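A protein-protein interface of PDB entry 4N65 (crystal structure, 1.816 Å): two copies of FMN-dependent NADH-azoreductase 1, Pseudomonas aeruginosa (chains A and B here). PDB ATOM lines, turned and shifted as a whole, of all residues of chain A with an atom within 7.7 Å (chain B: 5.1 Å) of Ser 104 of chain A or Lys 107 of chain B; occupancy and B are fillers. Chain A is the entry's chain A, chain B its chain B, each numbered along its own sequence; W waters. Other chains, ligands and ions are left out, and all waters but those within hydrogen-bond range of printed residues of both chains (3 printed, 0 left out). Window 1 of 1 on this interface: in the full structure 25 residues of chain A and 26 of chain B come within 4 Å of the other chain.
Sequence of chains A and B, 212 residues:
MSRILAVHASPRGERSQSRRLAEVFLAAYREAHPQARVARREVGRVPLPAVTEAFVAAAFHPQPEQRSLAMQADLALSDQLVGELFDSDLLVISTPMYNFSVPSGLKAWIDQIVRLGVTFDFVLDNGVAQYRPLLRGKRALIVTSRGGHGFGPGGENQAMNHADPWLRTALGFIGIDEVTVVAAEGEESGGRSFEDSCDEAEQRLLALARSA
Val 51 of chain B touches Pro 11 of chain A (O to CG, 3.5 Å).
CG1 of Val 51 of chain B touches CE2 of Tyr 98 of chain A, at 3.8 Å.
CB of Asn 99 of chain A touches CG2 of Ile 110 of chain B (3.97 Å).
NE1 of Trp 166 of chain B touches CB of Phe 100 of chain A, at 3.8 Å.
NE1 of Trp 166 of chain B touches CB of Ser 101 of chain A, at 3.6 Å.
Ser 104 of chain A touches Ala 50 of chain B (OG to CB, 3.3 Å).
N of Ala 108 of chain B touches CB of Ser 104 of chain A, at 3.6 Å.
Ala 108 of chain A touches Ser 104 of chain B.
Ser 104 of chain B touches Asp 111 of chain A (N to OD2, 3.8 Å).
CG of His 162 of chain A touches CB of Trp 166 of chain B, at 3.7 Å.
Ala 50 of chain A touches Ser 104 of chain B, and with the chains exchanged Ser 104 of chain A touches Ala 50 of chain B.
Ser 104 of chain A touches its own counterpart, Ser 104 of chain B.
Ser 104 of chain A touches Lys 107 of chain B, and with the chains exchanged Lys 107 of chain A touches Ser 104 of chain B.
Ser 104 of chain A touches Asp 111 of chain B, and with the chains exchanged Asp 111 of chain A touches Ser 104 of chain B.
Of the 21 pairs that touch across the chains among the printed residues, 11 have their exchanged pair printed and touching as well.
N of His 162 of chain A sits at hydrogen-bond distance from O of Phe 100 of chain A.
O of His 162 of chain A lies within hydrogen-bond range of OG of Ser 101 of chain A (3.4 Å).
The side-chain amino group (NZ) of Lys 107 of chain A is in salt-bridge range of the side-chain carboxylate (OD1) of Asp 111 of chain A (2.8 Å).
The side-chain amino group (NZ) of Lys 107 of chain B is in salt-bridge range of the side-chain carboxylate (OD1) of Asp 111 of chain B, 2.8 Å away.
Water W2 lies within hydrogen-bond range of OD2 of Asp 111 of chain B (2.6 Å), OG of Ser 104 of chain A (2.8 Å) and N of Val 51 of chain B (3.4 Å).
Water W1 lies within hydrogen-bond range of OD2 of Asp 111 of chain A (2.7 Å) and OG of Ser 104 of chain B (2.8 Å).
Water W3 lies within hydrogen-bond range of the backbone carbonyl oxygen of Asp 111 of chain B (2.7 Å) and the side-chain amide nitrogen of Asn 99 of chain A (3.0 Å).
Printed residues of chain B within 4 Å of Ser 104 of chain A: Ala 50 (3.3 Å), Ser 104 (3.5 Å), Lys 107 (3.8 Å), Ala 108 (3.6 Å) and Asp 111 (3.8 Å).
Lys 107 of chain B touches just these residues of chain A: Tyr 98 (2.9 Å), Ser 101 (3.9 Å), Val 102 (2.7 Å) and Ser 104 (3.8 Å).
Of the printed residues of chain A, Asp 111 of chain B touches Asn 99 and Ser 104.
Of the printed residues of chain A, Val 51 of chain B touches Pro 11 and Tyr 98.
Of the printed residues of chain A, Ile 110 of chain B touches Asn 99 (3.97 Å).
Printed residues of chain A within 4 Å of Val 102 of chain B: Lys 107 (2.7 Å).
Pro 103 of chain B touches none of the printed residues of chain A.
Trp 109 of chain B touches none of the printed residues of chain A.
The nearest residue of chain B that does not touch Ser 104 of chain A is Val 51 of chain B (4.9 Å).
The nearest residue of chain A that does not touch Lys 107 of chain B is Pro 103 of chain A (4.3 Å).
The backbone carbonyl oxygen of Tyr 98 of chain A sits at hydrogen-bond distance from the side-chain amino group of Lys 107 of chain B (2.9 Å).
OD1 of Asp 111 of chain B is in hydrogen-bond range of ND2 of Asn 99 of chain A (2.9 Å).
The indole nitrogen (NE1) of Trp 166 of chain B sits at hydrogen-bond distance from the backbone carbonyl oxygen (O) of Asn 99 of chain A, 2.8 Å away.
The backbone carbonyl oxygen of Val 102 of chain A is in hydrogen-bond range of the side-chain amino group of Lys 107 of chain B, at 2.7 Å.
The side-chain amino group (NZ) of Lys 107 of chain A is in hydrogen-bond range of the backbone carbonyl oxygen (O) of Val 102 of chain B, 2.7 Å away.
Printed residues of chain B that touch a printed residue of chain A: Ala 50, Val 51, Val 102, Ser 104, Lys 107, Ala 108, Ile 110, Asp 111 and Trp 166.
Hydrophobic or aromatic side chains of chain A within 4 Å of the printed part of chain B: Pro 11, Ala 50, Tyr 98, Phe 100, Ala 108 and His 162.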
ATOM      1  N   ALA A   9      31.083  26.614  17.268  1.00  0.00           N
ATOM      2  CA  ALA A   9      30.249  25.538  16.732  1.00  0.00           C
ATOM      3  C   ALA A   9      29.412  24.791  17.760  1.00  0.00           C
ATOM      4  O   ALA A   9      28.539  24.023  17.393  1.00  0.00           O
ATOM      5  CB  ALA A   9      31.102  24.542  15.916  1.00  0.00           C
ATOM      6  N   PRO A  11      26.326  24.138  20.020  1.00  0.00           N
ATOM      7  CA  PRO A  11      25.005  24.744  20.265  1.00  0.00           C
ATOM      8  C   PRO A  11      24.797  25.239  21.682  1.00  0.00           C
ATOM      9  O   PRO A  11      23.837  25.965  21.916  1.00  0.00           O
ATOM     10  CB  PRO A  11      24.002  23.628  19.922  1.00  0.00           C
ATOM     11  CG  PRO A  11      24.790  22.372  19.910  1.00  0.00           C
ATOM     12  CD  PRO A  11      26.270  22.680  19.845  1.00  0.00           C
ATOM     13  N   VAL A  43      28.060  29.420  14.456  1.00  0.00           N
ATOM     14  CA  VAL A  43      27.512  28.321  13.653  1.00  0.00           C
ATOM     15  C   VAL A  43      26.883  27.207  14.501  1.00  0.00           C
ATOM     16  O   VAL A  43      26.403  26.221  13.957  1.00  0.00           O
ATOM     17  CB  VAL A  43      28.542  27.777  12.629  1.00  0.00           C
ATOM     18  CG1 VAL A  43      29.166  28.947  11.812  1.00  0.00           C
ATOM     19  CG2 VAL A  43      29.626  26.930  13.262  1.00  0.00           C
ATOM     20  N   LEU A  48      23.071  27.268  10.285  1.00  0.00           N
ATOM     21  CA  LEU A  48      23.757  27.671   9.082  1.00  0.00           C
ATOM     22  C   LEU A  48      23.253  26.763   7.963  1.00  0.00           C
ATOM     23  O   LEU A  48      23.379  25.547   8.075  1.00  0.00           O
ATOM     24  CB  LEU A  48      25.258  27.533   9.297  1.00  0.00           C
ATOM     25  CG  LEU A  48      26.131  28.439   8.447  1.00  0.00           C
ATOM     26  CD1 LEU A  48      25.920  29.896   8.794  1.00  0.00           C
ATOM     27  CD2 LEU A  48      27.551  28.077   8.621  1.00  0.00           C
ATOM     28  N   PRO A  49      22.681  27.336   6.891  1.00  0.00           N
ATOM     29  CA  PRO A  49      22.112  26.474   5.844  1.00  0.00           C
ATOM     30  C   PRO A  49      23.085  25.489   5.210  1.00  0.00           C
ATOM     31  O   PRO A  49      24.227  25.796   4.961  1.00  0.00           O
ATOM     32  CB  PRO A  49      21.630  27.451   4.783  1.00  0.00           C
ATOM     33  CG  PRO A  49      22.253  28.732   5.096  1.00  0.00           C
ATOM     34  CD  PRO A  49      22.499  28.755   6.577  1.00  0.00           C
ATOM     35  N   ALA A  50      22.576  24.315   4.896  1.00  0.00           N
ATOM     36  CA  ALA A  50      23.326  23.356   4.094  1.00  0.00           C
ATOM     37  C   ALA A  50      23.437  23.772   2.635  1.00  0.00           C
ATOM     38  O   ALA A  50      22.635  24.568   2.104  1.00  0.00           O
ATOM     39  CB  ALA A  50      22.658  21.978   4.189  1.00  0.00           C
ATOM     40  N   THR A  95      34.795  23.806  18.792  1.00  0.00           N
ATOM     41  CA  THR A  95      33.864  22.734  18.474  1.00  0.00           C
ATOM     42  C   THR A  95      33.857  21.587  19.476  1.00  0.00           C
ATOM     43  O   THR A  95      34.900  21.108  19.898  1.00  0.00           O
ATOM     44  CB  THR A  95      34.110  22.175  17.043  1.00  0.00           C
ATOM     45  OG1 THR A  95      33.072  21.257  16.714  1.00  0.00           O
ATOM     46  CG2 THR A  95      35.472  21.489  16.893  1.00  0.00           C
ATOM     47  N   PRO A  96      32.663  21.123  19.841  1.00  0.00           N
ATOM     48  CA  PRO A  96      32.558  19.806  20.458  1.00  0.00           C
ATOM     49  C   PRO A  96      32.947  18.697  19.493  1.00  0.00           C
ATOM     50  O   PRO A  96      32.909  18.897  18.261  1.00  0.00           O
ATOM     51  CB  PRO A  96      31.061  19.647  20.679  1.00  0.00           C
ATOM     52  CG  PRO A  96      30.455  21.000  20.553  1.00  0.00           C
ATOM     53  CD  PRO A  96      31.350  21.750  19.630  1.00  0.00           C
ATOM     54  N   MET A  97      33.177  17.512  20.032  1.00  0.00           N
ATOM     55  CA  MET A  97      33.041  16.305  19.241  1.00  0.00           C
ATOM     56  C   MET A  97      31.614  15.801  19.392  1.00  0.00           C
ATOM     57  O   MET A  97      31.174  15.495  20.485  1.00  0.00           O
ATOM     58  CB  MET A  97      34.017  15.218  19.686  1.00  0.00           C
ATOM     59  CG  MET A  97      33.798  13.887  18.968  1.00  0.00           C
ATOM     60  SD  MET A  97      35.012  12.613  19.382  1.00  0.00           S
ATOM     61  CE  MET A  97      36.427  13.143  18.428  1.00  0.00           C
ATOM     62  N   TYR A  98      30.916  15.688  18.266  1.00  0.00           N
ATOM     63  CA  TYR A  98      29.583  15.096  18.248  1.00  0.00           C
ATOM     64  C   TYR A  98      29.609  13.860  17.362  1.00  0.00           C
ATOM     65  O   TYR A  98      29.861  13.980  16.160  1.00  0.00           O
ATOM     66  CB  TYR A  98      28.576  16.071  17.634  1.00  0.00           C
ATOM     67  CG  TYR A  98      27.931  17.068  18.582  1.00  0.00           C
ATOM     68  CD1 TYR A  98      28.373  17.227  19.894  1.00  0.00           C
ATOM     69  CD2 TYR A  98      26.869  17.858  18.159  1.00  0.00           C
ATOM     70  CE1 TYR A  98      27.774  18.143  20.746  1.00  0.00           C
ATOM     71  CE2 TYR A  98      26.260  18.769  19.019  1.00  0.00           C
ATOM     72  CZ  TYR A  98      26.723  18.908  20.306  1.00  0.00           C
ATOM     73  OH  TYR A  98      26.091  19.795  21.157  1.00  0.00           O
ATOM     74  N   ASN A  99      29.344  12.690  17.965  1.00  0.00           N
ATOM     75  CA  ASN A  99      29.311  11.420  17.246  1.00  0.00           C
ATOM     76  C   ASN A  99      30.533  11.238  16.324  1.00  0.00           C
ATOM     77  O   ASN A  99      30.423  10.944  15.141  1.00  0.00           O
ATOM     78  CB  ASN A  99      27.947  11.317  16.549  1.00  0.00           C
ATOM     79  CG  ASN A  99      26.812  11.316  17.570  1.00  0.00           C
ATOM     80  OD1 ASN A  99      26.873  10.582  18.550  1.00  0.00           O
ATOM     81  ND2 ASN A  99      25.838  12.177  17.392  1.00  0.00           N
ATOM     82  N   PHE A 100      31.704  11.414  16.929  1.00  0.00           N
ATOM     83  CA  PHE A 100      33.002  11.207  16.286  1.00  0.00           C
ATOM     84  C   PHE A 100      33.365  12.230  15.219  1.00  0.00           C
ATOM     85  O   PHE A 100      34.414  12.108  14.594  1.00  0.00           O
ATOM     86  CB  PHE A 100      33.112   9.779  15.754  1.00  0.00           C
ATOM     87  CG  PHE A 100      32.712   8.771  16.775  1.00  0.00           C
ATOM     88  CD1 PHE A 100      33.530   8.525  17.875  1.00  0.00           C
ATOM     89  CD2 PHE A 100      31.483   8.126  16.696  1.00  0.00           C
ATOM     90  CE1 PHE A 100      33.151   7.622  18.855  1.00  0.00           C
ATOM     91  CE2 PHE A 100      31.111   7.212  17.658  1.00  0.00           C
ATOM     92  CZ  PHE A 100      31.938   6.968  18.743  1.00  0.00           C
ATOM     93  N   SER A 101      32.538  13.264  15.057  1.00  0.00           N
ATOM     94  CA  SER A 101      32.835  14.316  14.113  1.00  0.00           C
ATOM     95  C   SER A 101      32.475  15.647  14.762  1.00  0.00           C
ATOM     96  O   SER A 101      32.575  15.788  15.997  1.00  0.00           O
ATOM     97  CB  SER A 101      32.067  14.046  12.821  1.00  0.00           C
ATOM     98  OG  SER A 101      32.371  14.972  11.797  1.00  0.00           O
ATOM     99  N   VAL A 102      32.083  16.614  13.950  1.00  0.00           N
ATOM    100  CA  VAL A 102      31.709  17.942  14.440  1.00  0.00           C
ATOM    101  C   VAL A 102      30.196  18.125  14.330  1.00  0.00           C
ATOM    102  O   VAL A 102      29.534  17.420  13.550  1.00  0.00           O
ATOM    103  CB  VAL A 102      32.432  19.078  13.665  1.00  0.00           C
ATOM    104  CG1 VAL A 102      33.965  18.938  13.799  1.00  0.00           C
ATOM    105  CG2 VAL A 102      31.991  19.139  12.207  1.00  0.00           C
ATOM    106  N   PRO A 103      29.647  19.085  15.091  1.00  0.00           N
ATOM    107  CA  PRO A 103      28.237  19.396  14.894  1.00  0.00           C
ATOM    108  C   PRO A 103      27.941  19.796  13.442  1.00  0.00           C
ATOM    109  O   PRO A 103      28.809  20.366  12.735  1.00  0.00           O
ATOM    110  CB  PRO A 103      27.983  20.564  15.854  1.00  0.00           C
ATOM    111  CG  PRO A 103      29.103  20.443  16.893  1.00  0.00           C
ATOM    112  CD  PRO A 103      30.276  19.956  16.112  1.00  0.00           C
ATOM    113  N   SER A 104      26.732  19.476  12.993  1.00  0.00           N
ATOM    114  CA  SER A 104      26.393  19.636  11.585  1.00  0.00           C
ATOM    115  C   SER A 104      26.518  21.085  11.102  1.00  0.00           C
ATOM    116  O   SER A 104      26.872  21.311   9.936  1.00  0.00           O
ATOM    117  CB  SER A 104      25.006  19.090  11.291  1.00  0.00           C
ATOM    118  OG  SER A 104      24.014  19.744  12.039  1.00  0.00           O
ATOM    119  N   GLY A 105      26.257  22.059  11.975  1.00  0.00           N
ATOM    120  CA  GLY A 105      26.394  23.468  11.618  1.00  0.00           C
ATOM    121  C   GLY A 105      27.806  23.842  11.164  1.00  0.00           C
ATOM    122  O   GLY A 105      27.981  24.674  10.264  1.00  0.00           O
ATOM    123  N   LEU A 106      28.811  23.213  11.762  1.00  0.00           N
ATOM    124  CA  LEU A 106      30.190  23.493  11.403  1.00  0.00           C
ATOM    125  C   LEU A 106      30.551  22.840  10.090  1.00  0.00           C
ATOM    126  O   LEU A 106      31.326  23.394   9.305  1.00  0.00           O
ATOM    127  CB  LEU A 106      31.169  23.038  12.494  1.00  0.00           C
ATOM    128  CG  LEU A 106      32.666  23.263  12.208  1.00  0.00           C
ATOM    129  CD1 LEU A 106      32.958  24.729  11.918  1.00  0.00           C
ATOM    130  CD2 LEU A 106      33.502  22.760  13.433  1.00  0.00           C
ATOM    131  N   LYS A 107      30.026  21.642   9.869  1.00  0.00           N
ATOM    132  CA  LYS A 107      30.121  21.043   8.535  1.00  0.00           C
ATOM    133  C   LYS A 107      29.492  21.942   7.488  1.00  0.00           C
ATOM    134  O   LYS A 107      30.028  22.057   6.383  1.00  0.00           O
ATOM    135  CB  LYS A 107      29.508  19.633   8.508  1.00  0.00           C
ATOM    136  CG  LYS A 107      29.574  18.931   7.154  1.00  0.00           C
ATOM    137  CD  LYS A 107      30.887  18.254   6.941  1.00  0.00           C
ATOM    138  CE  LYS A 107      31.521  18.543   5.621  1.00  0.00           C
ATOM    139  NZ  LYS A 107      30.795  18.228   4.357  1.00  0.00           N
ATOM    140  N   ALA A 108      28.358  22.572   7.797  1.00  0.00           N
ATOM    141  CA  ALA A 108      27.681  23.435   6.822  1.00  0.00           C
ATOM    142  C   ALA A 108      28.555  24.657   6.560  1.00  0.00           C
ATOM    143  O   ALA A 108      28.625  25.136   5.439  1.00  0.00           O
ATOM    144  CB  ALA A 108      26.330  23.842   7.321  1.00  0.00           C
ATOM    145  N   TRP A 109      29.219  25.149   7.597  1.00  0.00           N
ATOM    146  CA  TRP A 109      30.115  26.298   7.437  1.00  0.00           C
ATOM    147  C   TRP A 109      31.250  25.963   6.455  1.00  0.00           C
ATOM    148  O   TRP A 109      31.498  26.712   5.494  1.00  0.00           O
ATOM    149  CB  TRP A 109      30.670  26.759   8.785  1.00  0.00           C
ATOM    150  CG  TRP A 109      31.547  27.981   8.673  1.00  0.00           C
ATOM    151  CD1 TRP A 109      31.147  29.269   8.536  1.00  0.00           C
ATOM    152  CD2 TRP A 109      32.976  28.013   8.689  1.00  0.00           C
ATOM    153  NE1 TRP A 109      32.234  30.108   8.457  1.00  0.00           N
ATOM    154  CE2 TRP A 109      33.373  29.360   8.556  1.00  0.00           C
ATOM    155  CE3 TRP A 109      33.952  27.033   8.794  1.00  0.00           C
ATOM    156  CZ2 TRP A 109      34.701  29.747   8.502  1.00  0.00           C
ATOM    157  CZ3 TRP A 109      35.274  27.413   8.754  1.00  0.00           C
ATOM    158  CH2 TRP A 109      35.637  28.765   8.627  1.00  0.00           C
ATOM    159  N   ILE A 110      31.929  24.831   6.677  1.00  0.00           N
ATOM    160  CA  ILE A 110      32.985  24.389   5.769  1.00  0.00           C
ATOM    161  C   ILE A 110      32.438  24.295   4.354  1.00  0.00           C
ATOM    162  O   ILE A 110      33.054  24.760   3.396  1.00  0.00           O
ATOM    163  CB  ILE A 110      33.554  23.030   6.222  1.00  0.00           C
ATOM    164  CG1 ILE A 110      34.394  23.233   7.508  1.00  0.00           C
ATOM    165  CG2 ILE A 110      34.360  22.367   5.129  1.00  0.00           C
ATOM    166  CD1 ILE A 110      35.766  23.953   7.311  1.00  0.00           C
ATOM    167  N   ASP A 111      31.268  23.689   4.212  1.00  0.00           N
ATOM    168  CA  ASP A 111      30.669  23.533   2.869  1.00  0.00           C
ATOM    169  C   ASP A 111      30.339  24.849   2.162  1.00  0.00           C
ATOM    170  O   ASP A 111      30.291  24.890   0.901  1.00  0.00           O
ATOM    171  CB  ASP A 111      29.415  22.631   2.939  1.00  0.00           C
ATOM    172  CG  ASP A 111      29.738  21.169   3.248  1.00  0.00           C
ATOM    173  OD1 ASP A 111      30.904  20.746   3.124  1.00  0.00           O
ATOM    174  OD2 ASP A 111      28.787  20.428   3.627  1.00  0.00           O
ATOM    175  N   HIS A 162      37.096  11.730  13.870  1.00  0.00           N
ATOM    176  CA  HIS A 162      36.874  12.368  12.586  1.00  0.00           C
ATOM    177  C   HIS A 162      36.409  13.800  12.789  1.00  0.00           C
ATOM    178  O   HIS A 162      35.682  14.345  11.960  1.00  0.00           O
ATOM    179  CB  HIS A 162      35.863  11.566  11.780  1.00  0.00           C
ATOM    180  CG  HIS A 162      36.308  10.154  11.515  1.00  0.00           C
ATOM    181  ND1 HIS A 162      37.086   9.804  10.438  1.00  0.00           N
ATOM    182  CD2 HIS A 162      36.094   9.016  12.216  1.00  0.00           C
ATOM    183  CE1 HIS A 162      37.327   8.507  10.472  1.00  0.00           C
ATOM    184  NE2 HIS A 162      36.758   8.006  11.543  1.00  0.00           N
ATOM    185  N   ALA B  50      19.840  20.817  13.044  1.00  0.00           N
ATOM    186  CA  ALA B  50      20.984  20.483  13.887  1.00  0.00           C
ATOM    187  C   ALA B  50      20.516  20.275  15.306  1.00  0.00           C
ATOM    188  O   ALA B  50      19.488  20.825  15.725  1.00  0.00           O
ATOM    189  CB  ALA B  50      22.018  21.637  13.857  1.00  0.00           C
ATOM    190  N   VAL B  51      21.277  19.476  16.043  1.00  0.00           N
ATOM    191  CA  VAL B  51      21.161  19.387  17.499  1.00  0.00           C
ATOM    192  C   VAL B  51      21.290  20.755  18.117  1.00  0.00           C
ATOM    193  O   VAL B  51      22.198  21.515  17.786  1.00  0.00           O
ATOM    194  CB  VAL B  51      22.244  18.443  18.047  1.00  0.00           C
ATOM    195  CG1 VAL B  51      22.543  18.651  19.570  1.00  0.00           C
ATOM    196  CG2 VAL B  51      21.793  17.054  17.785  1.00  0.00           C
ATOM    197  N   VAL B 102      30.797  14.123   4.793  1.00  0.00           N
ATOM    198  CA  VAL B 102      29.467  14.014   4.190  1.00  0.00           C
ATOM    199  C   VAL B 102      28.762  15.370   4.209  1.00  0.00           C
ATOM    200  O   VAL B 102      29.141  16.248   4.977  1.00  0.00           O
ATOM    201  CB  VAL B 102      28.582  12.986   4.962  1.00  0.00           C
ATOM    202  CG1 VAL B 102      29.231  11.596   4.929  1.00  0.00           C
ATOM    203  CG2 VAL B 102      28.353  13.428   6.382  1.00  0.00           C
ATOM    204  N   PRO B 103      27.723  15.533   3.383  1.00  0.00           N
ATOM    205  CA  PRO B 103      26.938  16.764   3.453  1.00  0.00           C
ATOM    206  C   PRO B 103      26.375  16.954   4.860  1.00  0.00           C
ATOM    207  O   PRO B 103      26.155  15.990   5.603  1.00  0.00           O
ATOM    208  CB  PRO B 103      25.824  16.540   2.422  1.00  0.00           C
ATOM    209  CG  PRO B 103      26.368  15.469   1.483  1.00  0.00           C
ATOM    210  CD  PRO B 103      27.189  14.590   2.376  1.00  0.00           C
ATOM    211  N   SER B 104      26.175  18.211   5.244  1.00  0.00           N
ATOM    212  CA  SER B 104      25.860  18.517   6.625  1.00  0.00           C
ATOM    213  C   SER B 104      24.521  17.916   7.056  1.00  0.00           C
ATOM    214  O   SER B 104      24.371  17.578   8.224  1.00  0.00           O
ATOM    215  CB  SER B 104      25.860  20.032   6.886  1.00  0.00           C
ATOM    216  OG  SER B 104      24.979  20.718   6.022  1.00  0.00           O
ATOM    217  N   GLY B 105      23.560  17.778   6.133  1.00  0.00           N
ATOM    218  CA  GLY B 105      22.290  17.156   6.488  1.00  0.00           C
ATOM    219  C   GLY B 105      22.425  15.717   6.997  1.00  0.00           C
ATOM    220  O   GLY B 105      21.668  15.286   7.857  1.00  0.00           O
ATOM    221  N   LEU B 106      23.374  14.955   6.462  1.00  0.00           N
ATOM    222  CA  LEU B 106      23.564  13.590   6.904  1.00  0.00           C
ATOM    223  C   LEU B 106      24.239  13.585   8.283  1.00  0.00           C
ATOM    224  O   LEU B 106      23.972  12.712   9.103  1.00  0.00           O
ATOM    225  CB  LEU B 106      24.422  12.821   5.903  1.00  0.00           C
ATOM    226  CG  LEU B 106      24.707  11.349   6.198  1.00  0.00           C
ATOM    227  CD1 LEU B 106      23.424  10.564   6.519  1.00  0.00           C
ATOM    228  CD2 LEU B 106      25.452  10.734   5.054  1.00  0.00           C
ATOM    229  N   LYS B 107      25.133  14.537   8.514  1.00  0.00           N
ATOM    230  CA  LYS B 107      25.719  14.661   9.863  1.00  0.00           C
ATOM    231  C   LYS B 107      24.572  14.940  10.839  1.00  0.00           C
ATOM    232  O   LYS B 107      24.525  14.394  11.939  1.00  0.00           O
ATOM    233  CB  LYS B 107      26.762  15.778   9.922  1.00  0.00           C
ATOM    234  CG  LYS B 107      27.376  15.943  11.314  1.00  0.00           C
ATOM    235  CD  LYS B 107      28.334  14.786  11.596  1.00  0.00           C
ATOM    236  CE  LYS B 107      28.173  14.207  12.964  1.00  0.00           C
ATOM    237  NZ  LYS B 107      28.217  15.155  14.128  1.00  0.00           N
ATOM    238  N   ALA B 108      23.657  15.814  10.438  1.00  0.00           N
ATOM    239  CA  ALA B 108      22.494  16.142  11.260  1.00  0.00           C
ATOM    240  C   ALA B 108      21.611  14.907  11.566  1.00  0.00           C
ATOM    241  O   ALA B 108      21.155  14.725  12.684  1.00  0.00           O
ATOM    242  CB  ALA B 108      21.670  17.232  10.576  1.00  0.00           C
ATOM    243  N   TRP B 109      21.349  14.093  10.541  1.00  0.00           N
ATOM    244  CA  TRP B 109      20.620  12.836  10.709  1.00  0.00           C
ATOM    245  C   TRP B 109      21.281  11.932  11.759  1.00  0.00           C
ATOM    246  O   TRP B 109      20.627  11.497  12.694  1.00  0.00           O
ATOM    247  CB  TRP B 109      20.501  12.108   9.354  1.00  0.00           C
ATOM    248  CG  TRP B 109      19.676  10.879   9.456  1.00  0.00           C
ATOM    249  CD1 TRP B 109      18.319  10.812   9.573  1.00  0.00           C
ATOM    250  CD2 TRP B 109      20.156   9.519   9.520  1.00  0.00           C
ATOM    251  NE1 TRP B 109      17.921   9.504   9.685  1.00  0.00           N
ATOM    252  CE2 TRP B 109      19.022   8.690   9.650  1.00  0.00           C
ATOM    253  CE3 TRP B 109      21.420   8.933   9.459  1.00  0.00           C
ATOM    254  CZ2 TRP B 109      19.120   7.311   9.744  1.00  0.00           C
ATOM    255  CZ3 TRP B 109      21.516   7.535   9.536  1.00  0.00           C
ATOM    256  CH2 TRP B 109      20.372   6.754   9.688  1.00  0.00           C
ATOM    257  N   ILE B 110      22.583  11.678  11.637  1.00  0.00           N
ATOM    258  CA  ILE B 110      23.297  10.904  12.633  1.00  0.00           C
ATOM    259  C   ILE B 110      23.151  11.522  14.026  1.00  0.00           C
ATOM    260  O   ILE B 110      22.923  10.794  14.997  1.00  0.00           O
ATOM    261  CB  ILE B 110      24.797  10.754  12.263  1.00  0.00           C
ATOM    262  CG1 ILE B 110      24.926   9.826  11.055  1.00  0.00           C
ATOM    263  CG2 ILE B 110      25.642  10.296  13.488  1.00  0.00           C
ATOM    264  CD1 ILE B 110      24.688   8.356  11.354  1.00  0.00           C
ATOM    265  N   ASP B 111      23.282  12.847  14.124  1.00  0.00           N
ATOM    266  CA  ASP B 111      23.178  13.524  15.419  1.00  0.00           C
ATOM    267  C   ASP B 111      21.784  13.378  16.040  1.00  0.00           C
ATOM    268  O   ASP B 111      21.650  13.450  17.244  1.00  0.00           O
ATOM    269  CB  ASP B 111      23.584  15.013  15.328  1.00  0.00           C
ATOM    270  CG  ASP B 111      25.087  15.201  15.108  1.00  0.00           C
ATOM    271  OD1 ASP B 111      25.829  14.213  15.301  1.00  0.00           O
ATOM    272  OD2 ASP B 111      25.511  16.324  14.716  1.00  0.00           O
ATOM    273  N   TRP B 166      33.898   7.406   8.560  1.00  0.00           N
ATOM    274  CA  TRP B 166      33.252   8.029   9.710  1.00  0.00           C
ATOM    275  C   TRP B 166      31.843   7.442   9.917  1.00  0.00           C
ATOM    276  O   TRP B 166      31.425   7.126  11.043  1.00  0.00           O
ATOM    277  CB  TRP B 166      33.204   9.566   9.589  1.00  0.00           C
ATOM    278  CG  TRP B 166      32.231  10.087  10.579  1.00  0.00           C
ATOM    279  CD1 TRP B 166      32.398  10.153  11.931  1.00  0.00           C
ATOM    280  CD2 TRP B 166      30.884  10.468  10.320  1.00  0.00           C
ATOM    281  NE1 TRP B 166      31.237  10.562  12.529  1.00  0.00           N
ATOM    282  CE2 TRP B 166      30.297  10.781  11.560  1.00  0.00           C
ATOM    283  CE3 TRP B 166      30.118  10.594   9.154  1.00  0.00           C
ATOM    284  CZ2 TRP B 166      28.982  11.193  11.668  1.00  0.00           C
ATOM    285  CZ3 TRP B 166      28.810  11.026   9.275  1.00  0.00           C
ATOM    286  CH2 TRP B 166      28.261  11.309  10.521  1.00  0.00           C
HETATM  287  O   HOH W   1      26.179  20.984   3.547  1.00  0.00           O
HETATM  288  O   HOH W   2      24.175  18.601  14.552  1.00  0.00           O
HETATM  289  O   HOH W   3      23.393  12.464  19.049  1.00  0.00           O
